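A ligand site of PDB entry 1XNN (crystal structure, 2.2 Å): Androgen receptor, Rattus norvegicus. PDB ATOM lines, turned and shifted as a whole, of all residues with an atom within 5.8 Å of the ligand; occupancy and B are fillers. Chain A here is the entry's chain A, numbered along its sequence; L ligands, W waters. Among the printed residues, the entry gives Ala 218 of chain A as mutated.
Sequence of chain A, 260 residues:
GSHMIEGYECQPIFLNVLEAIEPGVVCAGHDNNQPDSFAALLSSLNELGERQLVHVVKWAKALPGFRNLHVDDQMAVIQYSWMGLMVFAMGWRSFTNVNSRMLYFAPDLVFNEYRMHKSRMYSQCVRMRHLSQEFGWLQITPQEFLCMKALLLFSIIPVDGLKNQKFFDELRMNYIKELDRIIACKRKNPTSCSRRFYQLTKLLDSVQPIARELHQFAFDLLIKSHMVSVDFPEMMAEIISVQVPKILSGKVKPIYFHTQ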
ATOM      1  N   LEU A  42      20.062   1.219  23.980  1.00  0.00           N
ATOM      2  CA  LEU A  42      19.154   2.292  23.599  1.00  0.00           C
ATOM      3  C   LEU A  42      18.118   1.877  22.561  1.00  0.00           C
ATOM      4  O   LEU A  42      17.010   2.389  22.562  1.00  0.00           O
ATOM      5  CB  LEU A  42      19.948   3.511  23.121  1.00  0.00           C
ATOM      6  CG  LEU A  42      20.299   4.502  24.240  1.00  0.00           C
ATOM      7  CD1 LEU A  42      19.023   5.062  24.837  1.00  0.00           C
ATOM      8  CD2 LEU A  42      21.111   3.813  25.311  1.00  0.00           C
ATOM      9  N   LEU A  45      15.574   0.100  24.566  1.00  0.00           N
ATOM     10  CA  LEU A  45      14.829   1.075  25.363  1.00  0.00           C
ATOM     11  C   LEU A  45      13.815   1.812  24.501  1.00  0.00           C
ATOM     12  O   LEU A  45      12.679   2.038  24.928  1.00  0.00           O
ATOM     13  CB  LEU A  45      15.787   2.081  26.028  1.00  0.00           C
ATOM     14  CG  LEU A  45      16.553   1.620  27.279  1.00  0.00           C
ATOM     15  CD1 LEU A  45      17.600   2.639  27.683  1.00  0.00           C
ATOM     16  CD2 LEU A  45      15.560   1.392  28.417  1.00  0.00           C
ATOM     17  N   ASN A  46      14.206   2.187  23.294  1.00  0.00           N
ATOM     18  CA  ASN A  46      13.299   2.889  22.396  1.00  0.00           C
ATOM     19  C   ASN A  46      12.139   1.974  22.013  1.00  0.00           C
ATOM     20  O   ASN A  46      10.991   2.409  21.939  1.00  0.00           O
ATOM     21  CB  ASN A  46      14.028   3.358  21.123  1.00  0.00           C
ATOM     22  CG  ASN A  46      15.019   4.488  21.383  1.00  0.00           C
ATOM     23  OD1 ASN A  46      15.727   4.934  20.472  1.00  0.00           O
ATOM     24  ND2 ASN A  46      15.078   4.966  22.622  1.00  0.00           N
ATOM     25  N   LEU A  48      10.987  -0.596  23.802  1.00  0.00           N
ATOM     26  CA  LEU A  48      10.197  -0.756  25.014  1.00  0.00           C
ATOM     27  C   LEU A  48       9.359   0.520  25.223  1.00  0.00           C
ATOM     28  O   LEU A  48       8.185   0.456  25.587  1.00  0.00           O
ATOM     29  CB  LEU A  48      11.109  -0.990  26.226  1.00  0.00           C
ATOM     30  CG  LEU A  48      10.419  -1.068  27.593  1.00  0.00           C
ATOM     31  CD1 LEU A  48       9.395  -2.205  27.599  1.00  0.00           C
ATOM     32  CD2 LEU A  48      11.465  -1.257  28.681  1.00  0.00           C
ATOM     33  N   GLY A  49       9.983   1.671  24.977  1.00  0.00           N
ATOM     34  CA  GLY A  49       9.286   2.935  25.134  1.00  0.00           C
ATOM     35  C   GLY A  49       8.056   3.019  24.244  1.00  0.00           C
ATOM     36  O   GLY A  49       7.001   3.483  24.673  1.00  0.00           O
ATOM     37  N   GLU A  50       8.187   2.562  22.997  1.00  0.00           N
ATOM     38  CA  GLU A  50       7.060   2.575  22.069  1.00  0.00           C
ATOM     39  C   GLU A  50       5.950   1.632  22.610  1.00  0.00           C
ATOM     40  O   GLU A  50       4.761   1.970  22.607  1.00  0.00           O
ATOM     41  CB  GLU A  50       7.522   2.082  20.690  1.00  0.00           C
ATOM     42  CG  GLU A  50       6.451   2.132  19.600  1.00  0.00           C
ATOM     43  CD  GLU A  50       6.442   3.440  18.836  1.00  0.00           C
ATOM     44  OE1 GLU A  50       6.578   4.498  19.476  1.00  0.00           O
ATOM     45  OE2 GLU A  50       6.280   3.403  17.601  1.00  0.00           O
ATOM     46  N   GLN A  52       5.385   0.682  25.712  1.00  0.00           N
ATOM     47  CA  GLN A  52       4.810   1.274  26.910  1.00  0.00           C
ATOM     48  C   GLN A  52       3.847   2.424  26.534  1.00  0.00           C
ATOM     49  O   GLN A  52       2.799   2.601  27.153  1.00  0.00           O
ATOM     50  CB  GLN A  52       5.924   1.805  27.810  1.00  0.00           C
ATOM     51  CG  GLN A  52       5.619   1.751  29.287  1.00  0.00           C
ATOM     52  CD  GLN A  52       5.699   0.350  29.844  1.00  0.00           C
ATOM     53  OE1 GLN A  52       6.744  -0.297  29.769  1.00  0.00           O
ATOM     54  NE2 GLN A  52       4.604  -0.115  30.420  1.00  0.00           N
ATOM     55  N   TRP A  82       3.698  11.313  29.077  1.00  0.00           N
ATOM     56  CA  TRP A  82       4.225   9.980  28.784  1.00  0.00           C
ATOM     57  C   TRP A  82       5.547   9.620  29.524  1.00  0.00           C
ATOM     58  O   TRP A  82       5.640   8.560  30.154  1.00  0.00           O
ATOM     59  CB  TRP A  82       4.415   9.845  27.277  1.00  0.00           C
ATOM     60  CG  TRP A  82       5.218   8.663  26.867  1.00  0.00           C
ATOM     61  CD1 TRP A  82       4.954   7.348  27.128  1.00  0.00           C
ATOM     62  CD2 TRP A  82       6.424   8.679  26.104  1.00  0.00           C
ATOM     63  NE1 TRP A  82       5.923   6.540  26.567  1.00  0.00           N
ATOM     64  CE2 TRP A  82       6.843   7.334  25.938  1.00  0.00           C
ATOM     65  CE3 TRP A  82       7.209   9.701  25.544  1.00  0.00           C
ATOM     66  CZ2 TRP A  82       7.999   6.988  25.229  1.00  0.00           C
ATOM     67  CZ3 TRP A  82       8.351   9.356  24.845  1.00  0.00           C
ATOM     68  CH2 TRP A  82       8.736   8.005  24.702  1.00  0.00           C
ATOM     69  N   MET A  83       6.552  10.485  29.430  1.00  0.00           N
ATOM     70  CA  MET A  83       7.840  10.254  30.072  1.00  0.00           C
ATOM     71  C   MET A  83       7.737  10.187  31.618  1.00  0.00           C
ATOM     72  O   MET A  83       8.279   9.283  32.229  1.00  0.00           O
ATOM     73  CB  MET A  83       8.824  11.356  29.686  1.00  0.00           C
ATOM     74  CG  MET A  83      10.265  11.059  30.083  1.00  0.00           C
ATOM     75  SD  MET A  83      10.844   9.542  29.286  1.00  0.00           S
ATOM     76  CE  MET A  83      10.987  10.169  27.625  1.00  0.00           C
ATOM     77  N   MET A  86       6.151   7.011  32.722  1.00  0.00           N
ATOM     78  CA  MET A  86       7.040   5.859  32.610  1.00  0.00           C
ATOM     79  C   MET A  86       8.072   5.861  33.721  1.00  0.00           C
ATOM     80  O   MET A  86       8.473   4.797  34.203  1.00  0.00           O
ATOM     81  CB  MET A  86       7.779   5.859  31.268  1.00  0.00           C
ATOM     82  CG  MET A  86       6.908   5.546  30.054  1.00  0.00           C
ATOM     83  SD  MET A  86       7.948   4.850  28.764  1.00  0.00           S
ATOM     84  CE  MET A  86       9.036   6.212  28.446  1.00  0.00           C
ATOM     85  N   VAL A  87       8.524   7.045  34.105  1.00  0.00           N
ATOM     86  CA  VAL A  87       9.497   7.171  35.171  1.00  0.00           C
ATOM     87  C   VAL A  87       8.883   6.685  36.456  1.00  0.00           C
ATOM     88  O   VAL A  87       9.452   5.843  37.155  1.00  0.00           O
ATOM     89  CB  VAL A  87       9.935   8.648  35.363  1.00  0.00           C
ATOM     90  CG1 VAL A  87      10.807   8.781  36.614  1.00  0.00           C
ATOM     91  CG2 VAL A  87      10.692   9.145  34.145  1.00  0.00           C
ATOM     92  N   MET A  90       8.069   2.888  36.465  1.00  0.00           N
ATOM     93  CA  MET A  90       9.310   2.128  36.470  1.00  0.00           C
ATOM     94  C   MET A  90       9.969   2.218  37.847  1.00  0.00           C
ATOM     95  O   MET A  90      10.614   1.283  38.298  1.00  0.00           O
ATOM     96  CB  MET A  90      10.248   2.645  35.387  1.00  0.00           C
ATOM     97  CG  MET A  90      11.411   1.722  35.080  1.00  0.00           C
ATOM     98  SD  MET A  90      12.849   2.046  36.086  1.00  0.00           S
ATOM     99  CE  MET A  90      13.510   3.559  35.246  1.00  0.00           C
ATOM    100  N   ARG A  93       8.093  -0.350  39.824  1.00  0.00           N
ATOM    101  CA  ARG A  93       8.492  -1.704  39.477  1.00  0.00           C
ATOM    102  C   ARG A  93       9.831  -2.046  40.120  1.00  0.00           C
ATOM    103  O   ARG A  93      10.028  -3.149  40.604  1.00  0.00           O
ATOM    104  CB  ARG A  93       8.634  -1.868  37.956  1.00  0.00           C
ATOM    105  CG  ARG A  93       7.324  -1.980  37.200  1.00  0.00           C
ATOM    106  CD  ARG A  93       7.549  -2.628  35.826  1.00  0.00           C
ATOM    107  NE  ARG A  93       8.440  -1.828  34.982  1.00  0.00           N
ATOM    108  CZ  ARG A  93       8.107  -0.666  34.418  1.00  0.00           C
ATOM    109  NH1 ARG A  93       6.898  -0.149  34.593  1.00  0.00           N
ATOM    110  NH2 ARG A  93       8.992  -0.029  33.668  1.00  0.00           N
ATOM    111  N   TYR A 104      14.372  -1.572  36.950  1.00  0.00           N
ATOM    112  CA  TYR A 104      13.573  -2.606  36.298  1.00  0.00           C
ATOM    113  C   TYR A 104      12.751  -2.024  35.126  1.00  0.00           C
ATOM    114  O   TYR A 104      11.533  -1.904  35.239  1.00  0.00           O
ATOM    115  CB  TYR A 104      12.641  -3.217  37.339  1.00  0.00           C
ATOM    116  CG  TYR A 104      12.153  -4.628  37.063  1.00  0.00           C
ATOM    117  CD1 TYR A 104      12.779  -5.718  37.658  1.00  0.00           C
ATOM    118  CD2 TYR A 104      11.035  -4.862  36.276  1.00  0.00           C
ATOM    119  CE1 TYR A 104      12.286  -7.024  37.473  1.00  0.00           C
ATOM    120  CE2 TYR A 104      10.526  -6.141  36.087  1.00  0.00           C
ATOM    121  CZ  TYR A 104      11.159  -7.221  36.690  1.00  0.00           C
ATOM    122  OH  TYR A 104      10.635  -8.480  36.537  1.00  0.00           O
ATOM    123  N   PHE A 105      13.402  -1.662  34.039  1.00  0.00           N
ATOM    124  CA  PHE A 105      12.698  -1.126  32.884  1.00  0.00           C
ATOM    125  C   PHE A 105      11.715  -2.196  32.376  1.00  0.00           C
ATOM    126  O   PHE A 105      10.566  -1.887  32.031  1.00  0.00           O
ATOM    127  CB  PHE A 105      13.672  -0.745  31.756  1.00  0.00           C
ATOM    128  CG  PHE A 105      14.479   0.480  32.022  1.00  0.00           C
ATOM    129  CD1 PHE A 105      15.740   0.394  32.605  1.00  0.00           C
ATOM    130  CD2 PHE A 105      14.012   1.734  31.646  1.00  0.00           C
ATOM    131  CE1 PHE A 105      16.529   1.540  32.806  1.00  0.00           C
ATOM    132  CE2 PHE A 105      14.779   2.885  31.846  1.00  0.00           C
ATOM    133  CZ  PHE A 105      16.048   2.791  32.420  1.00  0.00           C
ATOM    134  N   ALA A 106      12.167  -3.445  32.354  1.00  0.00           N
ATOM    135  CA  ALA A 106      11.354  -4.568  31.914  1.00  0.00           C
ATOM    136  C   ALA A 106      11.921  -5.828  32.473  1.00  0.00           C
ATOM    137  O   ALA A 106      13.066  -5.861  32.895  1.00  0.00           O
ATOM    138  CB  ALA A 106      11.319  -4.631  30.387  1.00  0.00           C
ATOM    139  N   MET A 121      23.269   7.182  30.279  1.00  0.00           N
ATOM    140  CA  MET A 121      22.196   7.848  31.004  1.00  0.00           C
ATOM    141  C   MET A 121      22.395   7.708  32.497  1.00  0.00           C
ATOM    142  O   MET A 121      21.425   7.753  33.253  1.00  0.00           O
ATOM    143  CB  MET A 121      20.846   7.231  30.667  1.00  0.00           C
ATOM    144  CG  MET A 121      20.355   7.446  29.266  1.00  0.00           C
ATOM    145  SD  MET A 121      18.636   6.952  29.188  1.00  0.00           S
ATOM    146  CE  MET A 121      18.813   5.213  29.393  1.00  0.00           C
ATOM    147  N   MET A 128      16.357   8.558  38.799  1.00  0.00           N
ATOM    148  CA  MET A 128      15.250   7.606  38.821  1.00  0.00           C
ATOM    149  C   MET A 128      15.358   6.572  39.935  1.00  0.00           C
ATOM    150  O   MET A 128      14.375   6.271  40.598  1.00  0.00           O
ATOM    151  CB  MET A 128      15.139   6.903  37.455  1.00  0.00           C
ATOM    152  CG  MET A 128      14.836   7.857  36.309  1.00  0.00           C
ATOM    153  SD  MET A 128      14.470   7.065  34.742  1.00  0.00           S
ATOM    154  CE  MET A 128      16.108   6.851  34.098  1.00  0.00           C
ATOM    155  N   LEU A 214      15.164  13.529  31.094  1.00  0.00           N
ATOM    156  CA  LEU A 214      14.947  12.446  30.144  1.00  0.00           C
ATOM    157  C   LEU A 214      14.483  13.001  28.806  1.00  0.00           C
ATOM    158  O   LEU A 214      14.832  12.466  27.764  1.00  0.00           O
ATOM    159  CB  LEU A 214      13.911  11.469  30.700  1.00  0.00           C
ATOM    160  CG  LEU A 214      14.415  10.546  31.814  1.00  0.00           C
ATOM    161  CD1 LEU A 214      13.265   9.807  32.447  1.00  0.00           C
ATOM    162  CD2 LEU A 214      15.417   9.574  31.255  1.00  0.00           C
ATOM    163  N   PHE A 217      17.538  14.444  27.124  1.00  0.00           N
ATOM    164  CA  PHE A 217      18.366  13.355  26.633  1.00  0.00           C
ATOM    165  C   PHE A 217      17.719  12.683  25.415  1.00  0.00           C
ATOM    166  O   PHE A 217      18.415  12.310  24.466  1.00  0.00           O
ATOM    167  CB  PHE A 217      18.609  12.325  27.745  1.00  0.00           C
ATOM    168  CG  PHE A 217      19.377  11.109  27.291  1.00  0.00           C
ATOM    169  CD1 PHE A 217      18.719  10.034  26.705  1.00  0.00           C
ATOM    170  CD2 PHE A 217      20.762  11.057  27.415  1.00  0.00           C
ATOM    171  CE1 PHE A 217      19.422   8.929  26.251  1.00  0.00           C
ATOM    172  CE2 PHE A 217      21.473   9.945  26.962  1.00  0.00           C
ATOM    173  CZ  PHE A 217      20.807   8.879  26.385  1.00  0.00           C
ATOM    174  N   ALA A 218      16.399  12.509  25.437  1.00  0.00           N
ATOM    175  CA  ALA A 218      15.696  11.884  24.333  1.00  0.00           C
ATOM    176  C   ALA A 218      15.822  12.744  23.055  1.00  0.00           C
ATOM    177  O   ALA A 218      16.077  12.215  21.972  1.00  0.00           O
ATOM    178  CB  ALA A 218      14.227  11.685  24.690  1.00  0.00           C
ATOM    179  N   LEU A 221      19.401  12.682  21.635  1.00  0.00           N
ATOM    180  CA  LEU A 221      19.672  11.393  21.013  1.00  0.00           C
ATOM    181  C   LEU A 221      18.959  11.259  19.657  1.00  0.00           C
ATOM    182  O   LEU A 221      19.556  10.782  18.700  1.00  0.00           O
ATOM    183  CB  LEU A 221      19.249  10.258  21.945  1.00  0.00           C
ATOM    184  CG  LEU A 221      19.600   8.830  21.502  1.00  0.00           C
ATOM    185  CD1 LEU A 221      21.075   8.743  21.091  1.00  0.00           C
ATOM    186  CD2 LEU A 221      19.307   7.870  22.641  1.00  0.00           C
ATOM    187  N   PHE A 232      14.547   4.728  16.202  1.00  0.00           N
ATOM    188  CA  PHE A 232      13.484   5.364  16.952  1.00  0.00           C
ATOM    189  C   PHE A 232      12.158   4.961  16.337  1.00  0.00           C
ATOM    190  O   PHE A 232      11.905   5.235  15.175  1.00  0.00           O
ATOM    191  CB  PHE A 232      13.619   6.896  16.926  1.00  0.00           C
ATOM    192  CG  PHE A 232      14.567   7.440  17.959  1.00  0.00           C
ATOM    193  CD1 PHE A 232      15.947   7.390  17.767  1.00  0.00           C
ATOM    194  CD2 PHE A 232      14.088   7.975  19.157  1.00  0.00           C
ATOM    195  CE1 PHE A 232      16.834   7.867  18.744  1.00  0.00           C
ATOM    196  CE2 PHE A 232      14.961   8.453  20.144  1.00  0.00           C
ATOM    197  CZ  PHE A 232      16.341   8.398  19.933  1.00  0.00           C
ATOM    198  N   MET A 236       7.177   7.208  18.936  1.00  0.00           N
ATOM    199  CA  MET A 236       8.087   7.835  19.892  1.00  0.00           C
ATOM    200  C   MET A 236       8.865   8.984  19.215  1.00  0.00           C
ATOM    201  O   MET A 236       9.064  10.044  19.803  1.00  0.00           O
ATOM    202  CB  MET A 236       9.070   6.787  20.441  1.00  0.00           C
ATOM    203  CG  MET A 236       9.879   7.272  21.632  1.00  0.00           C
ATOM    204  SD  MET A 236      11.094   6.089  22.244  1.00  0.00           S
ATOM    205  CE  MET A 236      12.553   6.812  21.659  1.00  0.00           C
ATOM    206  N   ILE A 240       8.867  12.981  20.315  1.00  0.00           N
ATOM    207  CA  ILE A 240      10.132  13.606  20.652  1.00  0.00           C
ATOM    208  C   ILE A 240      10.479  14.856  19.820  1.00  0.00           C
ATOM    209  O   ILE A 240      11.125  15.776  20.325  1.00  0.00           O
ATOM    210  CB  ILE A 240      11.289  12.568  20.532  1.00  0.00           C
ATOM    211  CG1 ILE A 240      11.016  11.475  21.575  1.00  0.00           C
ATOM    212  CG2 ILE A 240      12.639  13.229  20.758  1.00  0.00           C
ATOM    213  CD1 ILE A 240      11.965  10.312  21.525  1.00  0.00           C
HETATM  214  C1  LIG L   1      13.616   6.079  25.295  1.00  0.00           C
HETATM  215  C2  LIG L   1      12.547   5.509  26.168  1.00  0.00           C
HETATM  216  O1  LIG L   1      11.370   5.517  25.813  1.00  0.00           O
HETATM  217  N1  LIG L   1      13.083   5.039  27.323  1.00  0.00           N
HETATM  218  C3  LIG L   1      12.396   4.323  28.248  1.00  0.00           C
HETATM  219  C4  LIG L   1      11.839   3.057  27.750  1.00  0.00           C
HETATM  220  C5  LIG L   1      10.990   2.280  28.618  1.00  0.00           C
HETATM  221  C6  LIG L   1      10.772   2.733  29.991  1.00  0.00           C
HETATM  222  N2  LIG L   1      10.030   1.908  30.755  1.00  0.00           N
HETATM  223  O2  LIG L   1      10.603   1.274  31.800  1.00  0.00           O
HETATM  224  O3  LIG L   1       8.756   1.510  30.433  1.00  0.00           O
HETATM  225  C7  LIG L   1      11.350   3.943  30.561  1.00  0.00           C
HETATM  226  C8  LIG L   1      11.172   4.338  31.954  1.00  0.00           C
HETATM  227  C9  LIG L   1      11.817   5.557  32.469  1.00  0.00           C
HETATM  228  C10 LIG L   1      12.632   6.401  31.588  1.00  0.00           C
HETATM  229  C11 LIG L   1      12.814   6.034  30.158  1.00  0.00           C
HETATM  230  C12 LIG L   1      12.211   4.801  29.624  1.00  0.00           C
HETATM  231  C13 LIG L   1      14.413   5.223  27.381  1.00  0.00           C
HETATM  232  O4  LIG L   1      15.167   4.971  28.314  1.00  0.00           O
HETATM  233  C14 LIG L   1      14.921   5.802  26.100  1.00  0.00           C
HETATM  234  C15 LIG L   1      15.692   7.128  26.377  1.00  0.00           C
HETATM  235  C16 LIG L   1      14.752   8.110  27.106  1.00  0.00           C
HETATM  236  C17 LIG L   1      13.484   8.386  26.321  1.00  0.00           C
HETATM  237  C18 LIG L   1      13.439   7.583  25.005  1.00  0.00           C
HETATM  238  C19 LIG L   1      14.682   8.049  24.232  1.00  0.00           C
HETATM  239  C20 LIG L   1      15.963   7.806  25.030  1.00  0.00           C
HETATM  240  O   HOH W   1       7.576   2.515  32.816  1.00  0.00           O
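Water W1 lies within hydrogen-bond range of the backbone carbonyl oxygen (O) of Met 86 (2.8 Å), an oxygen (O3) of the ligand (2.8 Å) and the guanidinium group (NH2) of Arg 93 (3.0 Å).
The side-chain amide oxygen of Gln 52 lies close to an oxygen (O3) of the ligand (2.8 Å). NH2 of Arg 93 is in hydrogen-bond range of O2 of the ligand, 2.8 Å away.
An oxygen (O2) of the ligand sits close to the backbone carbonyl oxygen of Phe 105, 3.2 Å away. An oxygen (O1) of the ligand lies close to the side-chain sulfur (SD) of Met 236 (3.6 Å). Residues that only touch the ligand: Leu 45, Asn 46, Met 83, Gly 49, Met 90, Met 86, Leu 48, Leu 214, Ala 218, Met 128, Trp 82, Met 121, Phe 217 and Val 87. Of the 25 residues printed, 18 come within 4 Å of the ligand.
The guanidinium group of Arg 93 is in hydrogen-bond range of the backbone carbonyl oxygen of Phe 105, at 2.9 Å. The guanidinium group (NE) of Arg 93 lies within hydrogen-bond range of the backbone carbonyl oxygen (O) of Tyr 104. ND2 of Asn 46 lies close to O of Leu 42 (3.2 Å). The indole nitrogen of Trp 82 lies within hydrogen-bond range of the side-chain sulfur of Met 86. The side-chain carboxylate of Glu 50 sits at hydrogen-bond distance from the backbone NH of Met 236, at 2.8 Å.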
